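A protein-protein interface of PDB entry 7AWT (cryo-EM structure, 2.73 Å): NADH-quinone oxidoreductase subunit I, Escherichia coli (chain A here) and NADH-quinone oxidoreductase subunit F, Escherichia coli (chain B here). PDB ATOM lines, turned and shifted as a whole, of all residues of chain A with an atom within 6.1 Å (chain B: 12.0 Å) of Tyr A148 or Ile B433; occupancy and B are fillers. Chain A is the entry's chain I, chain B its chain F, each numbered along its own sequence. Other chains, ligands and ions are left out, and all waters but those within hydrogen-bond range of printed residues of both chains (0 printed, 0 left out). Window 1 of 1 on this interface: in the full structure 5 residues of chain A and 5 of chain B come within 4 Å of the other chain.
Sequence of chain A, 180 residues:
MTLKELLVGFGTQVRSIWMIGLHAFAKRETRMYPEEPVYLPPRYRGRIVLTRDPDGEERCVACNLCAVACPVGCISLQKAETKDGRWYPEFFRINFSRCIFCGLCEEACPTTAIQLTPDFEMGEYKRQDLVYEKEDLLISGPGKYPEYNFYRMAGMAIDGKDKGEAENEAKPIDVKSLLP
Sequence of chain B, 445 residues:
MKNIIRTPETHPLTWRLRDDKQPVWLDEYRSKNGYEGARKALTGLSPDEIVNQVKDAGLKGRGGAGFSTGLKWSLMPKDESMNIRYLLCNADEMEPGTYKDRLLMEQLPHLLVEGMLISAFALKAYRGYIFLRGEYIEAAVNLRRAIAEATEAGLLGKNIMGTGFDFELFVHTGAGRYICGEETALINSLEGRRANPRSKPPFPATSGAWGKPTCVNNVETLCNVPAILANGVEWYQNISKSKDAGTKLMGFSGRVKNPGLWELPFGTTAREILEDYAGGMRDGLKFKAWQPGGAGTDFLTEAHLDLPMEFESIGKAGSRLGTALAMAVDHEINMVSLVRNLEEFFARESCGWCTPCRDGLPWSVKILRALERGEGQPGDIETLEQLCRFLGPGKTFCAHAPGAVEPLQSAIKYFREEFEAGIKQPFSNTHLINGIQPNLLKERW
A ring nitrogen (NE2) of His B431 sits at hydrogen-bond distance from the side-chain sulfur (SD) of Met A153 (3.8 Å).
Tyr A148 touches one residue of chain B.
Of chain A, only Tyr A148 comes within 4 Å of Ile B433.
No residue of chain B comes within 4 Å of Thr A112.
Pro A146 touches one residue of chain B.
No residue of chain B comes within 4 Å of Glu A147.
No residue of chain B comes within 4 Å of Asn A149.
Phe A150 touches none of the printed residues of chain B.
Met A153 touches just one residue of chain B: His B431 (3.8 Å).
Printed residues of chain A within 4 Å of His B431: Met A153 (3.8 Å).
Printed residues of chain A within 4 Å of Ile B436: Tyr A145.
Arg A59 touches none of the printed residues of chain B.
The nearest residue of chain A that does not touch Ile B433 is Tyr A145 (4.8 Å).
The nearest printed residue of chain A that does not touch His B431 is Tyr A148 (4.9 Å).
Of the 13 printed residues of chain B, 5 touch a printed residue of chain A.
Hydrophobic or aromatic side chains of chain B within 4 Å of the printed part of chain A: His B431, Ile B433 and Ile B436.
Hydrophobic or aromatic side chains of chain A within 4 Å of the printed part of chain B: Tyr A145, Pro A146, Tyr A148 and Met A153.
Among the printed residues, 5 pairs touch across the chains.
Among the printed residues, no Asp or Glu carboxylate lies within 4 Å of a Lys or Arg side-chain nitrogen of the other chain.
Among the printed residues, merely in contact across the chains: Tyr A145 with Gly B435 (3.7 Å), Tyr A145 with Ile B436 (3.5 Å), Pro A146 with Asn B434 (3.9 Å) and Tyr A148 with Ile B433 (3.9 Å).
NH1 of Arg A59 lies within hydrogen-bond range of O of Tyr A145, at 2.9 Å.
NH1 of Arg A59 is in hydrogen-bond range of O of Tyr A148, at 2.5 Å.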
ATOM      1  N   ASP A  53     -13.438  -6.981   1.647  1.00  0.00           N
ATOM      2  CA  ASP A  53     -13.616  -7.702   0.392  1.00  0.00           C
ATOM      3  C   ASP A  53     -12.675  -7.108  -0.655  1.00  0.00           C
ATOM      4  O   ASP A  53     -11.868  -6.229  -0.357  1.00  0.00           O
ATOM      5  CB  ASP A  53     -15.088  -7.656  -0.013  1.00  0.00           C
ATOM      6  CG  ASP A  53     -15.649  -6.259  -0.029  1.00  0.00           C
ATOM      7  OD1 ASP A  53     -14.865  -5.295   0.054  1.00  0.00           O
ATOM      8  OD2 ASP A  53     -16.886  -6.125  -0.125  1.00  0.00           O
ATOM      9  N   PRO A  54     -12.699  -7.616  -1.893  1.00  0.00           N
ATOM     10  CA  PRO A  54     -11.932  -6.948  -2.957  1.00  0.00           C
ATOM     11  C   PRO A  54     -12.182  -5.452  -3.060  1.00  0.00           C
ATOM     12  O   PRO A  54     -11.283  -4.710  -3.473  1.00  0.00           O
ATOM     13  CB  PRO A  54     -12.394  -7.686  -4.216  1.00  0.00           C
ATOM     14  CG  PRO A  54     -12.640  -9.064  -3.739  1.00  0.00           C
ATOM     15  CD  PRO A  54     -13.133  -8.960  -2.317  1.00  0.00           C
ATOM     16  N   ARG A  59     -15.984  -6.869   5.184  1.00  0.00           N
ATOM     17  CA  ARG A  59     -16.754  -8.068   4.964  1.00  0.00           C
ATOM     18  C   ARG A  59     -17.882  -8.364   5.946  1.00  0.00           C
ATOM     19  O   ARG A  59     -18.981  -8.679   5.544  1.00  0.00           O
ATOM     20  CB  ARG A  59     -15.834  -9.251   4.878  1.00  0.00           C
ATOM     21  CG  ARG A  59     -15.536  -9.643   3.467  1.00  0.00           C
ATOM     22  CD  ARG A  59     -14.356 -10.560   3.422  1.00  0.00           C
ATOM     23  NE  ARG A  59     -14.203 -11.116   2.102  1.00  0.00           N
ATOM     24  CZ  ARG A  59     -13.054 -11.547   1.631  1.00  0.00           C
ATOM     25  NH1 ARG A  59     -12.979 -12.050   0.424  1.00  0.00           N
ATOM     26  NH2 ARG A  59     -11.981 -11.476   2.377  1.00  0.00           N
ATOM     27  N   PRO A 110     -19.804 -17.024   7.663  1.00  0.00           N
ATOM     28  CA  PRO A 110     -20.274 -17.319   6.312  1.00  0.00           C
ATOM     29  C   PRO A 110     -19.849 -16.253   5.314  1.00  0.00           C
ATOM     30  O   PRO A 110     -20.062 -16.427   4.118  1.00  0.00           O
ATOM     31  CB  PRO A 110     -21.787 -17.280   6.472  1.00  0.00           C
ATOM     32  CG  PRO A 110     -22.006 -16.254   7.525  1.00  0.00           C
ATOM     33  CD  PRO A 110     -20.828 -16.326   8.456  1.00  0.00           C
ATOM     34  N   THR A 111     -19.259 -15.166   5.798  1.00  0.00           N
ATOM     35  CA  THR A 111     -18.828 -14.089   4.916  1.00  0.00           C
ATOM     36  C   THR A 111     -17.321 -13.881   4.900  1.00  0.00           C
ATOM     37  O   THR A 111     -16.848 -12.903   4.332  1.00  0.00           O
ATOM     38  CB  THR A 111     -19.500 -12.755   5.266  1.00  0.00           C
ATOM     39  OG1 THR A 111     -18.806 -12.145   6.354  1.00  0.00           O
ATOM     40  CG2 THR A 111     -20.949 -12.971   5.642  1.00  0.00           C
ATOM     41  N   THR A 112     -16.587 -14.788   5.524  1.00  0.00           N
ATOM     42  CA  THR A 112     -15.131 -14.767   5.580  1.00  0.00           C
ATOM     43  C   THR A 112     -14.545 -13.501   6.142  1.00  0.00           C
ATOM     44  O   THR A 112     -13.506 -13.054   5.718  1.00  0.00           O
ATOM     45  CB  THR A 112     -14.524 -14.963   4.209  1.00  0.00           C
ATOM     46  OG1 THR A 112     -14.981 -13.931   3.351  1.00  0.00           O
ATOM     47  CG2 THR A 112     -14.967 -16.259   3.650  1.00  0.00           C
ATOM     48  N   TYR A 145      -8.694 -15.431   1.920  1.00  0.00           N
ATOM     49  CA  TYR A 145      -9.470 -15.631   0.697  1.00  0.00           C
ATOM     50  C   TYR A 145      -9.616 -14.323  -0.029  1.00  0.00           C
ATOM     51  O   TYR A 145     -10.456 -13.517   0.315  1.00  0.00           O
ATOM     52  CB  TYR A 145     -10.849 -16.185   1.034  1.00  0.00           C
ATOM     53  CG  TYR A 145     -10.856 -17.020   2.287  1.00  0.00           C
ATOM     54  CD1 TYR A 145     -10.651 -16.438   3.519  1.00  0.00           C
ATOM     55  CD2 TYR A 145     -11.070 -18.383   2.243  1.00  0.00           C
ATOM     56  CE1 TYR A 145     -10.640 -17.181   4.672  1.00  0.00           C
ATOM     57  CE2 TYR A 145     -11.064 -19.134   3.399  1.00  0.00           C
ATOM     58  CZ  TYR A 145     -10.848 -18.517   4.610  1.00  0.00           C
ATOM     59  OH  TYR A 145     -10.840 -19.219   5.780  1.00  0.00           O
ATOM     60  N   PRO A 146      -8.857 -14.156  -1.102  1.00  0.00           N
ATOM     61  CA  PRO A 146      -8.753 -12.967  -1.916  1.00  0.00           C
ATOM     62  C   PRO A 146      -9.924 -12.493  -2.697  1.00  0.00           C
ATOM     63  O   PRO A 146     -10.084 -11.308  -2.750  1.00  0.00           O
ATOM     64  CB  PRO A 146      -7.690 -13.351  -2.902  1.00  0.00           C
ATOM     65  CG  PRO A 146      -6.830 -14.233  -2.126  1.00  0.00           C
ATOM     66  CD  PRO A 146      -7.819 -15.107  -1.460  1.00  0.00           C
ATOM     67  N   GLU A 147     -10.675 -13.346  -3.371  1.00  0.00           N
ATOM     68  CA  GLU A 147     -11.762 -12.840  -4.202  1.00  0.00           C
ATOM     69  C   GLU A 147     -13.182 -13.097  -3.769  1.00  0.00           C
ATOM     70  O   GLU A 147     -14.092 -12.853  -4.542  1.00  0.00           O
ATOM     71  CB  GLU A 147     -11.617 -13.395  -5.616  1.00  0.00           C
ATOM     72  CG  GLU A 147     -10.407 -12.892  -6.371  1.00  0.00           C
ATOM     73  CD  GLU A 147     -10.285 -13.533  -7.734  1.00  0.00           C
ATOM     74  OE1 GLU A 147     -11.026 -14.498  -8.011  1.00  0.00           O
ATOM     75  OE2 GLU A 147      -9.448 -13.067  -8.532  1.00  0.00           O
ATOM     76  N   TYR A 148     -13.406 -13.586  -2.564  1.00  0.00           N
ATOM     77  CA  TYR A 148     -14.778 -13.916  -2.207  1.00  0.00           C
ATOM     78  C   TYR A 148     -15.517 -12.660  -1.770  1.00  0.00           C
ATOM     79  O   TYR A 148     -15.021 -11.891  -0.942  1.00  0.00           O
ATOM     80  CB  TYR A 148     -14.835 -14.968  -1.101  1.00  0.00           C
ATOM     81  CG  TYR A 148     -16.252 -15.405  -0.812  1.00  0.00           C
ATOM     82  CD1 TYR A 148     -16.954 -16.186  -1.715  1.00  0.00           C
ATOM     83  CD2 TYR A 148     -16.897 -15.012   0.348  1.00  0.00           C
ATOM     84  CE1 TYR A 148     -18.248 -16.576  -1.464  1.00  0.00           C
ATOM     85  CE2 TYR A 148     -18.195 -15.398   0.605  1.00  0.00           C
ATOM     86  CZ  TYR A 148     -18.863 -16.178  -0.304  1.00  0.00           C
ATOM     87  OH  TYR A 148     -20.155 -16.564  -0.051  1.00  0.00           O
ATOM     88  N   ASN A 149     -16.703 -12.453  -2.334  1.00  0.00           N
ATOM     89  CA  ASN A 149     -17.550 -11.311  -2.011  1.00  0.00           C
ATOM     90  C   ASN A 149     -18.937 -11.848  -1.695  1.00  0.00           C
ATOM     91  O   ASN A 149     -19.661 -12.266  -2.603  1.00  0.00           O
ATOM     92  CB  ASN A 149     -17.599 -10.314  -3.168  1.00  0.00           C
ATOM     93  CG  ASN A 149     -18.028  -8.933  -2.727  1.00  0.00           C
ATOM     94  OD1 ASN A 149     -18.605  -8.759  -1.657  1.00  0.00           O
ATOM     95  ND2 ASN A 149     -17.742  -7.939  -3.556  1.00  0.00           N
ATOM     96  N   PHE A 150     -19.299 -11.852  -0.411  1.00  0.00           N
ATOM     97  CA  PHE A 150     -20.589 -12.401  -0.009  1.00  0.00           C
ATOM     98  C   PHE A 150     -21.731 -11.670  -0.693  1.00  0.00           C
ATOM     99  O   PHE A 150     -22.662 -12.295  -1.212  1.00  0.00           O
ATOM    100  CB  PHE A 150     -20.751 -12.329   1.505  1.00  0.00           C
ATOM    101  CG  PHE A 150     -22.148 -12.610   1.974  1.00  0.00           C
ATOM    102  CD1 PHE A 150     -22.622 -13.904   2.035  1.00  0.00           C
ATOM    103  CD2 PHE A 150     -22.984 -11.581   2.355  1.00  0.00           C
ATOM    104  CE1 PHE A 150     -23.903 -14.164   2.464  1.00  0.00           C
ATOM    105  CE2 PHE A 150     -24.263 -11.839   2.783  1.00  0.00           C
ATOM    106  CZ  PHE A 150     -24.721 -13.130   2.836  1.00  0.00           C
ATOM    107  N   MET A 153     -23.152 -12.667  -3.784  1.00  0.00           N
ATOM    108  CA  MET A 153     -23.970 -13.874  -3.696  1.00  0.00           C
ATOM    109  C   MET A 153     -25.359 -13.615  -3.142  1.00  0.00           C
ATOM    110  O   MET A 153     -26.314 -14.236  -3.569  1.00  0.00           O
ATOM    111  CB  MET A 153     -23.322 -14.900  -2.777  1.00  0.00           C
ATOM    112  CG  MET A 153     -21.931 -15.363  -3.137  1.00  0.00           C
ATOM    113  SD  MET A 153     -21.836 -16.426  -4.568  1.00  0.00           S
ATOM    114  CE  MET A 153     -23.489 -17.085  -4.626  1.00  0.00           C
ATOM    115  N   SER B 428     -20.958 -29.830 -12.844  1.00  0.00           N
ATOM    116  CA  SER B 428     -20.270 -28.923 -11.968  1.00  0.00           C
ATOM    117  C   SER B 428     -21.263 -27.878 -11.586  1.00  0.00           C
ATOM    118  O   SER B 428     -21.995 -27.366 -12.406  1.00  0.00           O
ATOM    119  CB  SER B 428     -19.028 -28.315 -12.594  1.00  0.00           C
ATOM    120  OG  SER B 428     -18.429 -27.398 -11.690  1.00  0.00           O
ATOM    121  N   ASN B 429     -21.241 -27.535 -10.323  1.00  0.00           N
ATOM    122  CA  ASN B 429     -22.158 -26.567  -9.816  1.00  0.00           C
ATOM    123  C   ASN B 429     -21.482 -25.492  -8.965  1.00  0.00           C
ATOM    124  O   ASN B 429     -22.014 -24.417  -8.831  1.00  0.00           O
ATOM    125  CB  ASN B 429     -23.145 -27.321  -8.987  1.00  0.00           C
ATOM    126  CG  ASN B 429     -24.320 -26.515  -8.670  1.00  0.00           C
ATOM    127  OD1 ASN B 429     -24.376 -25.358  -8.995  1.00  0.00           O
ATOM    128  ND2 ASN B 429     -25.274 -27.115  -8.033  1.00  0.00           N
ATOM    129  N   THR B 430     -20.303 -25.764  -8.408  1.00  0.00           N
ATOM    130  CA  THR B 430     -19.635 -24.765  -7.590  1.00  0.00           C
ATOM    131  C   THR B 430     -18.790 -23.849  -8.475  1.00  0.00           C
ATOM    132  O   THR B 430     -18.740 -23.995  -9.699  1.00  0.00           O
ATOM    133  CB  THR B 430     -18.779 -25.441  -6.522  1.00  0.00           C
ATOM    134  OG1 THR B 430     -17.770 -26.238  -7.153  1.00  0.00           O
ATOM    135  CG2 THR B 430     -19.637 -26.330  -5.641  1.00  0.00           C
ATOM    136  N   HIS B 431     -18.198 -22.829  -7.849  1.00  0.00           N
ATOM    137  CA  HIS B 431     -17.313 -21.906  -8.558  1.00  0.00           C
ATOM    138  C   HIS B 431     -15.863 -21.808  -8.072  1.00  0.00           C
ATOM    139  O   HIS B 431     -15.114 -20.956  -8.517  1.00  0.00           O
ATOM    140  CB  HIS B 431     -17.956 -20.555  -8.925  1.00  0.00           C
ATOM    141  CG  HIS B 431     -18.208 -19.636  -7.772  1.00  0.00           C
ATOM    142  ND1 HIS B 431     -17.201 -19.149  -6.972  1.00  0.00           N
ATOM    143  CD2 HIS B 431     -19.349 -19.053  -7.335  1.00  0.00           C
ATOM    144  CE1 HIS B 431     -17.715 -18.336  -6.066  1.00  0.00           C
ATOM    145  NE2 HIS B 431     -19.017 -18.260  -6.265  1.00  0.00           N
ATOM    146  N   LEU B 432     -15.467 -22.755  -7.230  1.00  0.00           N
ATOM    147  CA  LEU B 432     -14.103 -22.830  -6.694  1.00  0.00           C
ATOM    148  C   LEU B 432     -13.498 -21.706  -5.838  1.00  0.00           C
ATOM    149  O   LEU B 432     -12.403 -21.260  -6.113  1.00  0.00           O
ATOM    150  CB  LEU B 432     -13.156 -23.122  -7.858  1.00  0.00           C
ATOM    151  CG  LEU B 432     -11.675 -23.390  -7.611  1.00  0.00           C
ATOM    152  CD1 LEU B 432     -11.471 -24.307  -6.421  1.00  0.00           C
ATOM    153  CD2 LEU B 432     -11.050 -23.988  -8.856  1.00  0.00           C
ATOM    154  N   ILE B 433     -14.210 -21.240  -4.819  1.00  0.00           N
ATOM    155  CA  ILE B 433     -13.695 -20.209  -3.929  1.00  0.00           C
ATOM    156  C   ILE B 433     -12.208 -20.450  -3.699  1.00  0.00           C
ATOM    157  O   ILE B 433     -11.759 -21.595  -3.580  1.00  0.00           O
ATOM    158  CB  ILE B 433     -14.488 -20.193  -2.607  1.00  0.00           C
ATOM    159  CG1 ILE B 433     -15.940 -19.789  -2.856  1.00  0.00           C
ATOM    160  CG2 ILE B 433     -13.859 -19.250  -1.599  1.00  0.00           C
ATOM    161  CD1 ILE B 433     -16.901 -20.939  -2.907  1.00  0.00           C
ATOM    162  N   ASN B 434     -11.439 -19.361  -3.644  1.00  0.00           N
ATOM    163  CA  ASN B 434      -9.981 -19.459  -3.664  1.00  0.00           C
ATOM    164  C   ASN B 434      -9.444 -20.173  -2.427  1.00  0.00           C
ATOM    165  O   ASN B 434      -8.774 -21.206  -2.535  1.00  0.00           O
ATOM    166  CB  ASN B 434      -9.371 -18.064  -3.786  1.00  0.00           C
ATOM    167  CG  ASN B 434      -7.889 -18.101  -4.094  1.00  0.00           C
ATOM    168  OD1 ASN B 434      -7.074 -18.457  -3.245  1.00  0.00           O
ATOM    169  ND2 ASN B 434      -7.532 -17.725  -5.315  1.00  0.00           N
ATOM    170  N   GLY B 435      -9.471 -19.600  -1.299  1.00  0.00           N
ATOM    171  CA  GLY B 435      -8.915 -20.250  -0.147  1.00  0.00           C
ATOM    172  C   GLY B 435      -9.511 -21.511   0.401  1.00  0.00           C
ATOM    173  O   GLY B 435      -8.964 -22.016   1.291  1.00  0.00           O
ATOM    174  N   ILE B 436     -10.663 -21.992  -0.068  1.00  0.00           N
ATOM    175  CA  ILE B 436     -11.261 -23.236   0.409  1.00  0.00           C
ATOM    176  C   ILE B 436     -10.918 -24.364  -0.552  1.00  0.00           C
ATOM    177  O   ILE B 436     -11.001 -24.202  -1.776  1.00  0.00           O
ATOM    178  CB  ILE B 436     -12.786 -23.097   0.561  1.00  0.00           C
ATOM    179  CG1 ILE B 436     -13.134 -21.790   1.271  1.00  0.00           C
ATOM    180  CG2 ILE B 436     -13.352 -24.290   1.311  1.00  0.00           C
ATOM    181  CD1 ILE B 436     -13.179 -21.909   2.767  1.00  0.00           C
ATOM    182  N   GLN B 437     -10.539 -25.511   0.002  1.00  0.00           N
ATOM    183  CA  GLN B 437     -10.285 -26.708  -0.793  1.00  0.00           C
ATOM    184  C   GLN B 437     -11.579 -27.491  -0.974  1.00  0.00           C
ATOM    185  O   GLN B 437     -12.252 -27.796   0.017  1.00  0.00           O
ATOM    186  CB  GLN B 437      -9.237 -27.587  -0.129  1.00  0.00           C
ATOM    187  CG  GLN B 437      -7.833 -27.012  -0.177  1.00  0.00           C
ATOM    188  CD  GLN B 437      -6.909 -27.639   0.845  1.00  0.00           C
ATOM    189  OE1 GLN B 437      -5.927 -28.291   0.495  1.00  0.00           O
ATOM    190  NE2 GLN B 437      -7.222 -27.443   2.120  1.00  0.00           N
ATOM    191  N   PRO B 438     -11.960 -27.822  -2.206  1.00  0.00           N
ATOM    192  CA  PRO B 438     -13.246 -28.489  -2.426  1.00  0.00           C
ATOM    193  C   PRO B 438     -13.301 -29.860  -1.772  1.00  0.00           C
ATOM    194  O   PRO B 438     -12.284 -30.531  -1.589  1.00  0.00           O
ATOM    195  CB  PRO B 438     -13.333 -28.597  -3.953  1.00  0.00           C
ATOM    196  CG  PRO B 438     -12.412 -27.541  -4.463  1.00  0.00           C
ATOM    197  CD  PRO B 438     -11.293 -27.474  -3.472  1.00  0.00           C
ATOM    198  N   ASN B 439     -14.518 -30.269  -1.417  1.00  0.00           N
ATOM    199  CA  ASN B 439     -14.769 -31.599  -0.873  1.00  0.00           C
ATOM    200  C   ASN B 439     -14.837 -32.587  -2.029  1.00  0.00           C
ATOM    201  O   ASN B 439     -15.771 -32.545  -2.835  1.00  0.00           O
ATOM    202  CB  ASN B 439     -16.061 -31.603  -0.063  1.00  0.00           C
ATOM    203  CG  ASN B 439     -16.188 -32.822   0.824  1.00  0.00           C
ATOM    204  OD1 ASN B 439     -15.190 -33.386   1.266  1.00  0.00           O
ATOM    205  ND2 ASN B 439     -17.420 -33.233   1.090  1.00  0.00           N
ATOM    206  N   LEU B 440     -13.867 -33.469  -2.106  1.00  0.00           N
ATOM    207  CA  LEU B 440     -13.751 -34.409  -3.197  1.00  0.00           C
ATOM    208  C   LEU B 440     -14.732 -35.552  -3.149  1.00  0.00           C
ATOM    209  O   LEU B 440     -15.560 -35.622  -2.275  1.00  0.00           O
ATOM    210  CB  LEU B 440     -12.327 -34.923  -3.258  1.00  0.00           C
ATOM    211  CG  LEU B 440     -11.370 -33.753  -3.425  1.00  0.00           C
ATOM    212  CD1 LEU B 440      -9.938 -34.247  -3.529  1.00  0.00           C
ATOM    213  CD2 LEU B 440     -11.775 -32.976  -4.664  1.00  0.00           C
